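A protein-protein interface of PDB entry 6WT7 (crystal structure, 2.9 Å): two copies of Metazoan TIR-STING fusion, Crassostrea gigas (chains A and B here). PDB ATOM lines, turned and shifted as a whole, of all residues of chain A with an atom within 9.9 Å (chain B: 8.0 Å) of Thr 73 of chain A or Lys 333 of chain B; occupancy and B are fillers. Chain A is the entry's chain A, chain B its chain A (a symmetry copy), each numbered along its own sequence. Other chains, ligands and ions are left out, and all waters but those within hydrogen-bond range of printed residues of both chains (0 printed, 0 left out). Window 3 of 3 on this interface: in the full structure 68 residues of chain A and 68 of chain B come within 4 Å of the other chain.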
ATOM      1  N   PHE A  34      -2.334   3.256 -28.518  1.00  0.00           N
ATOM      2  CA  PHE A  34      -1.286   4.139 -28.025  1.00  0.00           C
ATOM      3  C   PHE A  34      -0.576   3.455 -26.867  1.00  0.00           C
ATOM      4  O   PHE A  34      -1.218   3.038 -25.898  1.00  0.00           O
ATOM      5  CB  PHE A  34      -1.860   5.484 -27.574  1.00  0.00           C
ATOM      6  CG  PHE A  34      -0.843   6.397 -26.940  1.00  0.00           C
ATOM      7  CD1 PHE A  34      -0.060   7.230 -27.721  1.00  0.00           C
ATOM      8  CD2 PHE A  34      -0.676   6.426 -25.563  1.00  0.00           C
ATOM      9  CE1 PHE A  34       0.873   8.072 -27.142  1.00  0.00           C
ATOM     10  CE2 PHE A  34       0.256   7.264 -24.980  1.00  0.00           C
ATOM     11  CZ  PHE A  34       1.030   8.089 -25.770  1.00  0.00           C
ATOM     12  N   ALA A  63       6.108   6.492 -28.712  1.00  0.00           N
ATOM     13  CA  ALA A  63       6.560   7.866 -28.510  1.00  0.00           C
ATOM     14  C   ALA A  63       7.953   8.099 -29.085  1.00  0.00           C
ATOM     15  O   ALA A  63       8.233   9.176 -29.626  1.00  0.00           O
ATOM     16  CB  ALA A  63       6.530   8.212 -27.020  1.00  0.00           C
ATOM     17  N   PHE A  67       6.876  10.689 -32.127  1.00  0.00           N
ATOM     18  CA  PHE A  67       6.898  12.060 -31.641  1.00  0.00           C
ATOM     19  C   PHE A  67       8.237  12.712 -31.961  1.00  0.00           C
ATOM     20  O   PHE A  67       9.260  12.039 -32.107  1.00  0.00           O
ATOM     21  CB  PHE A  67       6.657  12.123 -30.130  1.00  0.00           C
ATOM     22  CG  PHE A  67       5.279  11.700 -29.710  1.00  0.00           C
ATOM     23  CD1 PHE A  67       4.247  11.621 -30.631  1.00  0.00           C
ATOM     24  CD2 PHE A  67       5.016  11.386 -28.388  1.00  0.00           C
ATOM     25  CE1 PHE A  67       2.980  11.231 -30.239  1.00  0.00           C
ATOM     26  CE2 PHE A  67       3.753  10.997 -27.990  1.00  0.00           C
ATOM     27  CZ  PHE A  67       2.734  10.919 -28.916  1.00  0.00           C
ATOM     28  N   LEU A  68       8.219  14.037 -32.066  1.00  0.00           N
ATOM     29  CA  LEU A  68       9.462  14.776 -32.198  1.00  0.00           C
ATOM     30  C   LEU A  68      10.151  14.877 -30.836  1.00  0.00           C
ATOM     31  O   LEU A  68       9.491  14.800 -29.796  1.00  0.00           O
ATOM     32  CB  LEU A  68       9.198  16.169 -32.757  1.00  0.00           C
ATOM     33  CG  LEU A  68       8.460  16.214 -34.098  1.00  0.00           C
ATOM     34  CD1 LEU A  68       8.339  17.644 -34.604  1.00  0.00           C
ATOM     35  CD2 LEU A  68       9.154  15.330 -35.127  1.00  0.00           C
ATOM     36  N   PRO A  69      11.480  15.027 -30.817  1.00  0.00           N
ATOM     37  CA  PRO A  69      12.189  15.089 -29.523  1.00  0.00           C
ATOM     38  C   PRO A  69      11.661  16.161 -28.581  1.00  0.00           C
ATOM     39  O   PRO A  69      11.379  15.871 -27.411  1.00  0.00           O
ATOM     40  CB  PRO A  69      13.640  15.350 -29.944  1.00  0.00           C
ATOM     41  CG  PRO A  69      13.744  14.751 -31.306  1.00  0.00           C
ATOM     42  CD  PRO A  69      12.413  15.002 -31.958  1.00  0.00           C
ATOM     43  N   GLY A  70      11.515  17.394 -29.061  1.00  0.00           N
ATOM     44  CA  GLY A  70      10.976  18.456 -28.232  1.00  0.00           C
ATOM     45  C   GLY A  70       9.466  18.523 -28.175  1.00  0.00           C
ATOM     46  O   GLY A  70       8.924  19.251 -27.338  1.00  0.00           O
ATOM     47  N   GLU A  71       8.779  17.784 -29.037  1.00  0.00           N
ATOM     48  CA  GLU A  71       7.316  17.784 -29.093  1.00  0.00           C
ATOM     49  C   GLU A  71       6.728  16.587 -28.356  1.00  0.00           C
ATOM     50  O   GLU A  71       5.856  15.885 -28.868  1.00  0.00           O
ATOM     51  CB  GLU A  71       6.847  17.819 -30.542  1.00  0.00           C
ATOM     52  CG  GLU A  71       6.863  19.206 -31.164  1.00  0.00           C
ATOM     53  CD  GLU A  71       5.648  20.030 -30.780  1.00  0.00           C
ATOM     54  OE1 GLU A  71       4.727  20.159 -31.615  1.00  0.00           O
ATOM     55  OE2 GLU A  71       5.606  20.539 -29.641  1.00  0.00           O
ATOM     56  N   CYS A  72       7.205  16.339 -27.137  1.00  0.00           N
ATOM     57  CA  CYS A  72       6.650  15.311 -26.266  1.00  0.00           C
ATOM     58  C   CYS A  72       5.872  15.927 -25.107  1.00  0.00           C
ATOM     59  O   CYS A  72       5.836  15.373 -24.005  1.00  0.00           O
ATOM     60  CB  CYS A  72       7.755  14.391 -25.747  1.00  0.00           C
ATOM     61  SG  CYS A  72       7.176  12.811 -25.075  1.00  0.00           S
ATOM     62  N   THR A  73       5.247  17.077 -25.346  1.00  0.00           N
ATOM     63  CA  THR A  73       4.500  17.769 -24.310  1.00  0.00           C
ATOM     64  C   THR A  73       3.273  16.954 -23.898  1.00  0.00           C
ATOM     65  O   THR A  73       2.927  15.938 -24.508  1.00  0.00           O
ATOM     66  CB  THR A  73       4.079  19.158 -24.790  1.00  0.00           C
ATOM     67  OG1 THR A  73       3.212  19.032 -25.925  1.00  0.00           O
ATOM     68  CG2 THR A  73       5.300  19.979 -25.181  1.00  0.00           C
ATOM     69  N   SER A  74       2.608  17.419 -22.838  1.00  0.00           N
ATOM     70  CA  SER A  74       1.458  16.692 -22.310  1.00  0.00           C
ATOM     71  C   SER A  74       0.294  16.698 -23.295  1.00  0.00           C
ATOM     72  O   SER A  74      -0.412  15.694 -23.434  1.00  0.00           O
ATOM     73  CB  SER A  74       1.034  17.288 -20.968  1.00  0.00           C
ATOM     74  OG  SER A  74       2.098  17.244 -20.030  1.00  0.00           O
ATOM     75  N   ASP A  75       0.082  17.819 -23.992  1.00  0.00           N
ATOM     76  CA  ASP A  75      -1.020  17.896 -24.946  1.00  0.00           C
ATOM     77  C   ASP A  75      -0.776  17.015 -26.165  1.00  0.00           C
ATOM     78  O   ASP A  75      -1.728  16.462 -26.726  1.00  0.00           O
ATOM     79  CB  ASP A  75      -1.242  19.345 -25.378  1.00  0.00           C
ATOM     80  CG  ASP A  75       0.050  20.050 -25.730  1.00  0.00           C
ATOM     81  OD1 ASP A  75       1.022  19.919 -24.961  1.00  0.00           O
ATOM     82  OD2 ASP A  75       0.098  20.729 -26.777  1.00  0.00           O
ATOM     83  N   VAL A  76       0.481  16.880 -26.595  1.00  0.00           N
ATOM     84  CA  VAL A  76       0.786  16.014 -27.732  1.00  0.00           C
ATOM     85  C   VAL A  76       0.486  14.559 -27.389  1.00  0.00           C
ATOM     86  O   VAL A  76      -0.058  13.812 -28.212  1.00  0.00           O
ATOM     87  CB  VAL A  76       2.249  16.209 -28.173  1.00  0.00           C
ATOM     88  CG1 VAL A  76       2.687  15.070 -29.083  1.00  0.00           C
ATOM     89  CG2 VAL A  76       2.408  17.546 -28.878  1.00  0.00           C
ATOM     90  N   VAL A  77       0.829  14.136 -26.170  1.00  0.00           N
ATOM     91  CA  VAL A  77       0.461  12.799 -25.711  1.00  0.00           C
ATOM     92  C   VAL A  77      -1.053  12.643 -25.703  1.00  0.00           C
ATOM     93  O   VAL A  77      -1.587  11.578 -26.040  1.00  0.00           O
ATOM     94  CB  VAL A  77       1.069  12.531 -24.321  1.00  0.00           C
ATOM     95  CG1 VAL A  77       0.494  11.259 -23.713  1.00  0.00           C
ATOM     96  CG2 VAL A  77       2.585  12.444 -24.414  1.00  0.00           C
ATOM     97  N   VAL A  78      -1.771  13.708 -25.343  1.00  0.00           N
ATOM     98  CA  VAL A  78      -3.226  13.639 -25.257  1.00  0.00           C
ATOM     99  C   VAL A  78      -3.846  13.498 -26.644  1.00  0.00           C
ATOM    100  O   VAL A  78      -4.796  12.729 -26.836  1.00  0.00           O
ATOM    101  CB  VAL A  78      -3.763  14.870 -24.506  1.00  0.00           C
ATOM    102  CG1 VAL A  78      -5.251  15.036 -24.738  1.00  0.00           C
ATOM    103  CG2 VAL A  78      -3.473  14.736 -23.022  1.00  0.00           C
ATOM    104  N   ASP A  79      -3.321  14.230 -27.631  1.00  0.00           N
ATOM    105  CA  ASP A  79      -3.849  14.121 -28.989  1.00  0.00           C
ATOM    106  C   ASP A  79      -3.649  12.719 -29.549  1.00  0.00           C
ATOM    107  O   ASP A  79      -4.505  12.204 -30.276  1.00  0.00           O
ATOM    108  CB  ASP A  79      -3.193  15.158 -29.900  1.00  0.00           C
ATOM    109  CG  ASP A  79      -3.875  16.511 -29.826  1.00  0.00           C
ATOM    110  OD1 ASP A  79      -5.108  16.547 -29.623  1.00  0.00           O
ATOM    111  OD2 ASP A  79      -3.178  17.538 -29.971  1.00  0.00           O
ATOM    112  N   ALA A  80      -2.521  12.084 -29.223  1.00  0.00           N
ATOM    113  CA  ALA A  80      -2.303  10.708 -29.654  1.00  0.00           C
ATOM    114  C   ALA A  80      -3.313   9.765 -29.013  1.00  0.00           C
ATOM    115  O   ALA A  80      -3.781   8.816 -29.652  1.00  0.00           O
ATOM    116  CB  ALA A  80      -0.875  10.276 -29.325  1.00  0.00           C
ATOM    117  N   ILE A  81      -3.660  10.013 -27.747  1.00  0.00           N
ATOM    118  CA  ILE A  81      -4.684   9.212 -27.084  1.00  0.00           C
ATOM    119  C   ILE A  81      -6.047   9.462 -27.717  1.00  0.00           C
ATOM    120  O   ILE A  81      -6.833   8.528 -27.925  1.00  0.00           O
ATOM    121  CB  ILE A  81      -4.697   9.511 -25.574  1.00  0.00           C
ATOM    122  CG1 ILE A  81      -3.348   9.154 -24.950  1.00  0.00           C
ATOM    123  CG2 ILE A  81      -5.817   8.752 -24.884  1.00  0.00           C
ATOM    124  CD1 ILE A  81      -3.243   9.516 -23.489  1.00  0.00           C
ATOM    125  N   PHE A 103       1.174  11.306 -13.036  1.00  0.00           N
ATOM    126  CA  PHE A 103       0.920  12.418 -13.942  1.00  0.00           C
ATOM    127  C   PHE A 103       0.457  11.938 -15.314  1.00  0.00           C
ATOM    128  O   PHE A 103      -0.744  11.943 -15.604  1.00  0.00           O
ATOM    129  CB  PHE A 103       2.174  13.287 -14.078  1.00  0.00           C
ATOM    130  CG  PHE A 103       1.932  14.606 -14.757  1.00  0.00           C
ATOM    131  CD1 PHE A 103       1.147  15.574 -14.156  1.00  0.00           C
ATOM    132  CD2 PHE A 103       2.501  14.886 -15.988  1.00  0.00           C
ATOM    133  CE1 PHE A 103       0.924  16.792 -14.774  1.00  0.00           C
ATOM    134  CE2 PHE A 103       2.282  16.101 -16.613  1.00  0.00           C
ATOM    135  CZ  PHE A 103       1.492  17.055 -16.004  1.00  0.00           C
ATOM    136  N   GLU A 104       1.398  11.515 -16.162  1.00  0.00           N
ATOM    137  CA  GLU A 104       1.052  11.210 -17.548  1.00  0.00           C
ATOM    138  C   GLU A 104       0.310   9.885 -17.678  1.00  0.00           C
ATOM    139  O   GLU A 104      -0.494   9.720 -18.604  1.00  0.00           O
ATOM    140  CB  GLU A 104       2.311  11.203 -18.417  1.00  0.00           C
ATOM    141  CG  GLU A 104       2.995  12.558 -18.518  1.00  0.00           C
ATOM    142  CD  GLU A 104       4.108  12.583 -19.546  1.00  0.00           C
ATOM    143  OE1 GLU A 104       4.284  11.574 -20.261  1.00  0.00           O
ATOM    144  OE2 GLU A 104       4.805  13.615 -19.641  1.00  0.00           O
ATOM    145  N   MET A 107      -3.463  10.399 -17.330  1.00  0.00           N
ATOM    146  CA  MET A 107      -4.159  11.078 -18.416  1.00  0.00           C
ATOM    147  C   MET A 107      -4.760  10.100 -19.417  1.00  0.00           C
ATOM    148  O   MET A 107      -5.606  10.500 -20.224  1.00  0.00           O
ATOM    149  CB  MET A 107      -3.213  12.048 -19.125  1.00  0.00           C
ATOM    150  CG  MET A 107      -2.618  13.099 -18.201  1.00  0.00           C
ATOM    151  SD  MET A 107      -1.736  14.409 -19.071  1.00  0.00           S
ATOM    152  CE  MET A 107      -0.540  13.456 -20.001  1.00  0.00           C
ATOM    153  N   PHE B 220      -8.179  27.464 -24.731  1.00  0.00           N
ATOM    154  CA  PHE B 220      -7.928  26.529 -23.634  1.00  0.00           C
ATOM    155  C   PHE B 220      -6.491  26.745 -23.174  1.00  0.00           C
ATOM    156  O   PHE B 220      -5.576  26.023 -23.594  1.00  0.00           O
ATOM    157  CB  PHE B 220      -8.178  25.087 -24.092  1.00  0.00           C
ATOM    158  CG  PHE B 220      -8.239  24.062 -22.976  1.00  0.00           C
ATOM    159  CD1 PHE B 220      -7.565  24.246 -21.777  1.00  0.00           C
ATOM    160  CD2 PHE B 220      -8.966  22.895 -23.148  1.00  0.00           C
ATOM    161  CE1 PHE B 220      -7.622  23.293 -20.777  1.00  0.00           C
ATOM    162  CE2 PHE B 220      -9.027  21.939 -22.151  1.00  0.00           C
ATOM    163  CZ  PHE B 220      -8.355  22.139 -20.964  1.00  0.00           C
ATOM    164  N   PRO B 221      -6.256  27.730 -22.311  1.00  0.00           N
ATOM    165  CA  PRO B 221      -4.908  27.919 -21.765  1.00  0.00           C
ATOM    166  C   PRO B 221      -4.508  26.758 -20.868  1.00  0.00           C
ATOM    167  O   PRO B 221      -5.340  26.150 -20.189  1.00  0.00           O
ATOM    168  CB  PRO B 221      -5.025  29.225 -20.972  1.00  0.00           C
ATOM    169  CG  PRO B 221      -6.471  29.323 -20.625  1.00  0.00           C
ATOM    170  CD  PRO B 221      -7.206  28.728 -21.791  1.00  0.00           C
ATOM    171  N   GLN B 222      -3.208  26.456 -20.874  1.00  0.00           N
ATOM    172  CA  GLN B 222      -2.709  25.303 -20.130  1.00  0.00           C
ATOM    173  C   GLN B 222      -2.920  25.472 -18.631  1.00  0.00           C
ATOM    174  O   GLN B 222      -3.263  24.511 -17.933  1.00  0.00           O
ATOM    175  CB  GLN B 222      -1.230  25.082 -20.439  1.00  0.00           C
ATOM    176  CG  GLN B 222      -0.615  23.902 -19.708  1.00  0.00           C
ATOM    177  CD  GLN B 222       0.884  23.824 -19.894  1.00  0.00           C
ATOM    178  OE1 GLN B 222       1.634  24.604 -19.306  1.00  0.00           O
ATOM    179  NE2 GLN B 222       1.330  22.886 -20.722  1.00  0.00           N
ATOM    180  N   SER B 223      -2.717  26.683 -18.115  1.00  0.00           N
ATOM    181  CA  SER B 223      -2.873  26.950 -16.691  1.00  0.00           C
ATOM    182  C   SER B 223      -4.327  27.076 -16.263  1.00  0.00           C
ATOM    183  O   SER B 223      -4.587  27.231 -15.065  1.00  0.00           O
ATOM    184  CB  SER B 223      -2.128  28.231 -16.309  1.00  0.00           C
ATOM    185  OG  SER B 223      -2.846  29.375 -16.740  1.00  0.00           O
ATOM    186  N   GLU B 233      -5.006  40.130 -23.021  1.00  0.00           N
ATOM    187  CA  GLU B 233      -3.772  39.452 -23.396  1.00  0.00           C
ATOM    188  C   GLU B 233      -2.779  40.415 -24.035  1.00  0.00           C
ATOM    189  O   GLU B 233      -1.569  40.305 -23.806  1.00  0.00           O
ATOM    190  CB  GLU B 233      -4.075  38.294 -24.345  1.00  0.00           C
ATOM    191  CG  GLU B 233      -4.914  37.177 -23.735  1.00  0.00           C
ATOM    192  CD  GLU B 233      -4.092  36.196 -22.919  1.00  0.00           C
ATOM    193  OE1 GLU B 233      -2.899  36.472 -22.666  1.00  0.00           O
ATOM    194  OE2 GLU B 233      -4.640  35.142 -22.535  1.00  0.00           O
ATOM    195  N   TYR B 303      -3.307  19.873 -13.931  1.00  0.00           N
ATOM    196  CA  TYR B 303      -2.921  19.505 -15.287  1.00  0.00           C
ATOM    197  C   TYR B 303      -3.517  18.165 -15.692  1.00  0.00           C
ATOM    198  O   TYR B 303      -3.842  17.960 -16.867  1.00  0.00           O
ATOM    199  CB  TYR B 303      -1.397  19.470 -15.407  1.00  0.00           C
ATOM    200  CG  TYR B 303      -0.744  20.831 -15.322  1.00  0.00           C
ATOM    201  CD1 TYR B 303      -1.422  21.974 -15.728  1.00  0.00           C
ATOM    202  CD2 TYR B 303       0.552  20.975 -14.839  1.00  0.00           C
ATOM    203  CE1 TYR B 303      -0.831  23.220 -15.654  1.00  0.00           C
ATOM    204  CE2 TYR B 303       1.151  22.219 -14.763  1.00  0.00           C
ATOM    205  CZ  TYR B 303       0.455  23.337 -15.171  1.00  0.00           C
ATOM    206  OH  TYR B 303       1.044  24.579 -15.097  1.00  0.00           O
ATOM    207  N   MET B 307      -6.581  17.684 -18.620  1.00  0.00           N
ATOM    208  CA  MET B 307      -6.372  16.847 -19.797  1.00  0.00           C
ATOM    209  C   MET B 307      -7.445  15.774 -19.917  1.00  0.00           C
ATOM    210  O   MET B 307      -7.867  15.438 -21.029  1.00  0.00           O
ATOM    211  CB  MET B 307      -4.980  16.220 -19.757  1.00  0.00           C
ATOM    212  CG  MET B 307      -3.847  17.207 -20.000  1.00  0.00           C
ATOM    213  SD  MET B 307      -3.913  17.988 -21.626  1.00  0.00           S
ATOM    214  CE  MET B 307      -4.632  19.581 -21.233  1.00  0.00           C
ATOM    215  N   VAL B 330      -8.641  25.490 -29.021  1.00  0.00           N
ATOM    216  CA  VAL B 330      -7.249  25.891 -29.198  1.00  0.00           C
ATOM    217  C   VAL B 330      -6.564  25.770 -27.841  1.00  0.00           C
ATOM    218  O   VAL B 330      -6.726  26.639 -26.977  1.00  0.00           O
ATOM    219  CB  VAL B 330      -7.116  27.313 -29.753  1.00  0.00           C
ATOM    220  CG1 VAL B 330      -5.649  27.681 -29.928  1.00  0.00           C
ATOM    221  CG2 VAL B 330      -7.864  27.443 -31.070  1.00  0.00           C
ATOM    222  N   PHE B 331      -5.800  24.698 -27.647  1.00  0.00           N
ATOM    223  CA  PHE B 331      -4.978  24.552 -26.455  1.00  0.00           C
ATOM    224  C   PHE B 331      -3.613  25.180 -26.696  1.00  0.00           C
ATOM    225  O   PHE B 331      -3.071  25.113 -27.803  1.00  0.00           O
ATOM    226  CB  PHE B 331      -4.816  23.082 -26.068  1.00  0.00           C
ATOM    227  CG  PHE B 331      -3.965  22.871 -24.844  1.00  0.00           C
ATOM    228  CD1 PHE B 331      -4.523  22.937 -23.579  1.00  0.00           C
ATOM    229  CD2 PHE B 331      -2.606  22.620 -24.959  1.00  0.00           C
ATOM    230  CE1 PHE B 331      -3.743  22.752 -22.452  1.00  0.00           C
ATOM    231  CE2 PHE B 331      -1.823  22.437 -23.836  1.00  0.00           C
ATOM    232  CZ  PHE B 331      -2.392  22.501 -22.582  1.00  0.00           C
ATOM    233  N   TYR B 332      -3.057  25.783 -25.649  1.00  0.00           N
ATOM    234  CA  TYR B 332      -1.775  26.466 -25.756  1.00  0.00           C
ATOM    235  C   TYR B 332      -1.204  26.652 -24.359  1.00  0.00           C
ATOM    236  O   TYR B 332      -1.890  26.459 -23.353  1.00  0.00           O
ATOM    237  CB  TYR B 332      -1.919  27.815 -26.471  1.00  0.00           C
ATOM    238  CG  TYR B 332      -2.797  28.803 -25.735  1.00  0.00           C
ATOM    239  CD1 TYR B 332      -4.179  28.778 -25.878  1.00  0.00           C
ATOM    240  CD2 TYR B 332      -2.244  29.763 -24.894  1.00  0.00           C
ATOM    241  CE1 TYR B 332      -4.986  29.677 -25.204  1.00  0.00           C
ATOM    242  CE2 TYR B 332      -3.042  30.667 -24.217  1.00  0.00           C
ATOM    243  CZ  TYR B 332      -4.413  30.619 -24.375  1.00  0.00           C
ATOM    244  OH  TYR B 332      -5.211  31.517 -23.704  1.00  0.00           O
ATOM    245  N   LYS B 333       0.068  27.033 -24.313  1.00  0.00           N
ATOM    246  CA  LYS B 333       0.719  27.393 -23.064  1.00  0.00           C
ATOM    247  C   LYS B 333       0.637  28.899 -22.857  1.00  0.00           C
ATOM    248  O   LYS B 333       0.785  29.677 -23.803  1.00  0.00           O
ATOM    249  CB  LYS B 333       2.183  26.945 -23.053  1.00  0.00           C
ATOM    250  CG  LYS B 333       2.395  25.450 -22.865  1.00  0.00           C
ATOM    251  CD  LYS B 333       2.300  24.693 -24.181  1.00  0.00           C
ATOM    252  CE  LYS B 333       2.658  23.226 -23.995  1.00  0.00           C
ATOM    253  NZ  LYS B 333       2.634  22.478 -25.282  1.00  0.00           N
ATOM    254  N   ASP B 334       0.392  29.303 -21.612  1.00  0.00           N
ATOM    255  CA  ASP B 334       0.341  30.712 -21.240  1.00  0.00           C
ATOM    256  C   ASP B 334       1.340  31.027 -20.130  1.00  0.00           C
ATOM    257  O   ASP B 334       1.090  31.886 -19.283  1.00  0.00           O
ATOM    258  CB  ASP B 334      -1.075  31.113 -20.827  1.00  0.00           C
ATOM    259  CG  ASP B 334      -1.695  30.141 -19.840  1.00  0.00           C
ATOM    260  OD1 ASP B 334      -1.280  28.963 -19.818  1.00  0.00           O
ATOM    261  OD2 ASP B 334      -2.603  30.556 -19.090  1.00  0.00           O
ATOM    262  N   VAL B 335       2.482  30.336 -20.131  1.00  0.00           N
ATOM    263  CA  VAL B 335       3.476  30.541 -19.083  1.00  0.00           C
ATOM    264  C   VAL B 335       4.404  31.704 -19.420  1.00  0.00           C
ATOM    265  O   VAL B 335       4.917  32.373 -18.514  1.00  0.00           O
ATOM    266  CB  VAL B 335       4.267  29.244 -18.841  1.00  0.00           C
ATOM    267  CG1 VAL B 335       3.360  28.171 -18.253  1.00  0.00           C
ATOM    268  CG2 VAL B 335       4.902  28.755 -20.135  1.00  0.00           C
ATOM    269  N   ASN B 336       4.636  31.969 -20.702  1.00  0.00           N
ATOM    270  CA  ASN B 336       5.484  33.083 -21.088  1.00  0.00           C
ATOM    271  C   ASN B 336       4.718  34.400 -20.989  1.00  0.00           C
ATOM    272  O   ASN B 336       3.486  34.442 -21.041  1.00  0.00           O
ATOM    273  CB  ASN B 336       6.024  32.888 -22.506  1.00  0.00           C
ATOM    274  CG  ASN B 336       4.962  32.410 -23.475  1.00  0.00           C
ATOM    275  OD1 ASN B 336       3.794  32.262 -23.114  1.00  0.00           O
ATOM    276  ND2 ASN B 336       5.361  32.170 -24.718  1.00  0.00           N
ATOM    277  N   ALA B 341       2.921  36.736 -28.174  1.00  0.00           N
ATOM    278  CA  ALA B 341       2.673  35.315 -28.397  1.00  0.00           C
ATOM    279  C   ALA B 341       1.193  35.031 -28.620  1.00  0.00           C
ATOM    280  O   ALA B 341       0.831  34.217 -29.477  1.00  0.00           O
ATOM    281  CB  ALA B 341       3.200  34.498 -27.218  1.00  0.00           C
ATOM    282  N   MET B 342       0.322  35.688 -27.856  1.00  0.00           N
ATOM    283  CA  MET B 342      -1.114  35.463 -27.964  1.00  0.00           C
ATOM    284  C   MET B 342      -1.699  36.065 -29.243  1.00  0.00           C
ATOM    285  O   MET B 342      -2.503  35.399 -29.905  1.00  0.00           O
ATOM    286  CB  MET B 342      -1.837  36.016 -26.734  1.00  0.00           C
ATOM    287  CG  MET B 342      -3.310  35.655 -26.675  1.00  0.00           C
ATOM    288  SD  MET B 342      -3.570  33.875 -26.542  1.00  0.00           S
ATOM    289  CE  MET B 342      -5.354  33.797 -26.426  1.00  0.00           C
ATOM    290  N   LEU B 345      -0.805  33.885 -32.194  1.00  0.00           N
ATOM    291  CA  LEU B 345      -1.494  32.601 -32.118  1.00  0.00           C
ATOM    292  C   LEU B 345      -2.904  32.702 -32.680  1.00  0.00           C
ATOM    293  O   LEU B 345      -3.351  31.818 -33.420  1.00  0.00           O
ATOM    294  CB  LEU B 345      -1.524  32.106 -30.673  1.00  0.00           C
ATOM    295  CG  LEU B 345      -2.387  30.877 -30.377  1.00  0.00           C
ATOM    296  CD1 LEU B 345      -1.979  29.700 -31.249  1.00  0.00           C
ATOM    297  CD2 LEU B 345      -2.296  30.511 -28.906  1.00  0.00           C
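The side-chain carboxylate (OD1) of Asp 75 of chain A lies within salt-bridge range of the side-chain amino group (NZ) of Lys 333 of chain B (3.0 Å).
OG1 of Thr 73 of chain A is in hydrogen-bond range of OD1 of Asp 75 of chain A (2.6 Å).
OG1 of Thr 73 of chain A touches NZ of Lys 333 of chain B, at 3.6 Å. CB of Asp 75 of chain A touches CE2 of Phe 331 of chain B, 3.5 Å away. Val 78 of chain A touches Met 307 of chain B (CG2 to SD, 3.6 Å). CE1 of Phe 103 of chain A touches CB of Tyr 303 of chain B, 3.6 Å away. Met 107 of chain A touches Met 307 of chain B (SD to CG, 3.6 Å).
Of the printed residues of chain B, Thr 73 of chain A touches Lys 333. Printed residues of chain B within 4 Å of Asp 75 of chain A: Phe 331 and Lys 333. Of the printed residues of chain B, Phe 103 of chain A touches Tyr 303 (3.6 Å). Of the printed residues of chain B, Met 107 of chain A touches Met 307. Tyr 332 of chain B touches none of the printed residues of chain A. Of chain A, only Thr 73 and Asp 75 come within 4 Å of Lys 333 of chain B. Asp 334 of chain B touches none of the printed residues of chain A. The nearest printed residue of chain A that does not touch Lys 333 of chain B is Ser 74 of chain A (5.6 Å). The nearest printed residue of chain B that does not touch Val 78 of chain A is Tyr 303 of chain B (7.0 Å).
Of the 20 printed residues of chain A, 5 touch a printed residue of chain B. Printed residues of chain A that touch a printed residue of chain B: Thr 73, Asp 75, Val 78, Phe 103 and Met 107. Hydrophobic or aromatic side chains of chain A that line the printed part of chain B: Val 78, Phe 103 and Met 107. Along chain A the printed residues that touch a printed residue of chain B span positions 73 to 107. Of the 17 printed residues of chain B, 4 touch a printed residue of chain A. Hydrophobic or aromatic side chains of chain B that line the printed part of chain A: Tyr 303, Met 307 and Phe 331.
No position is printed for both chains.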
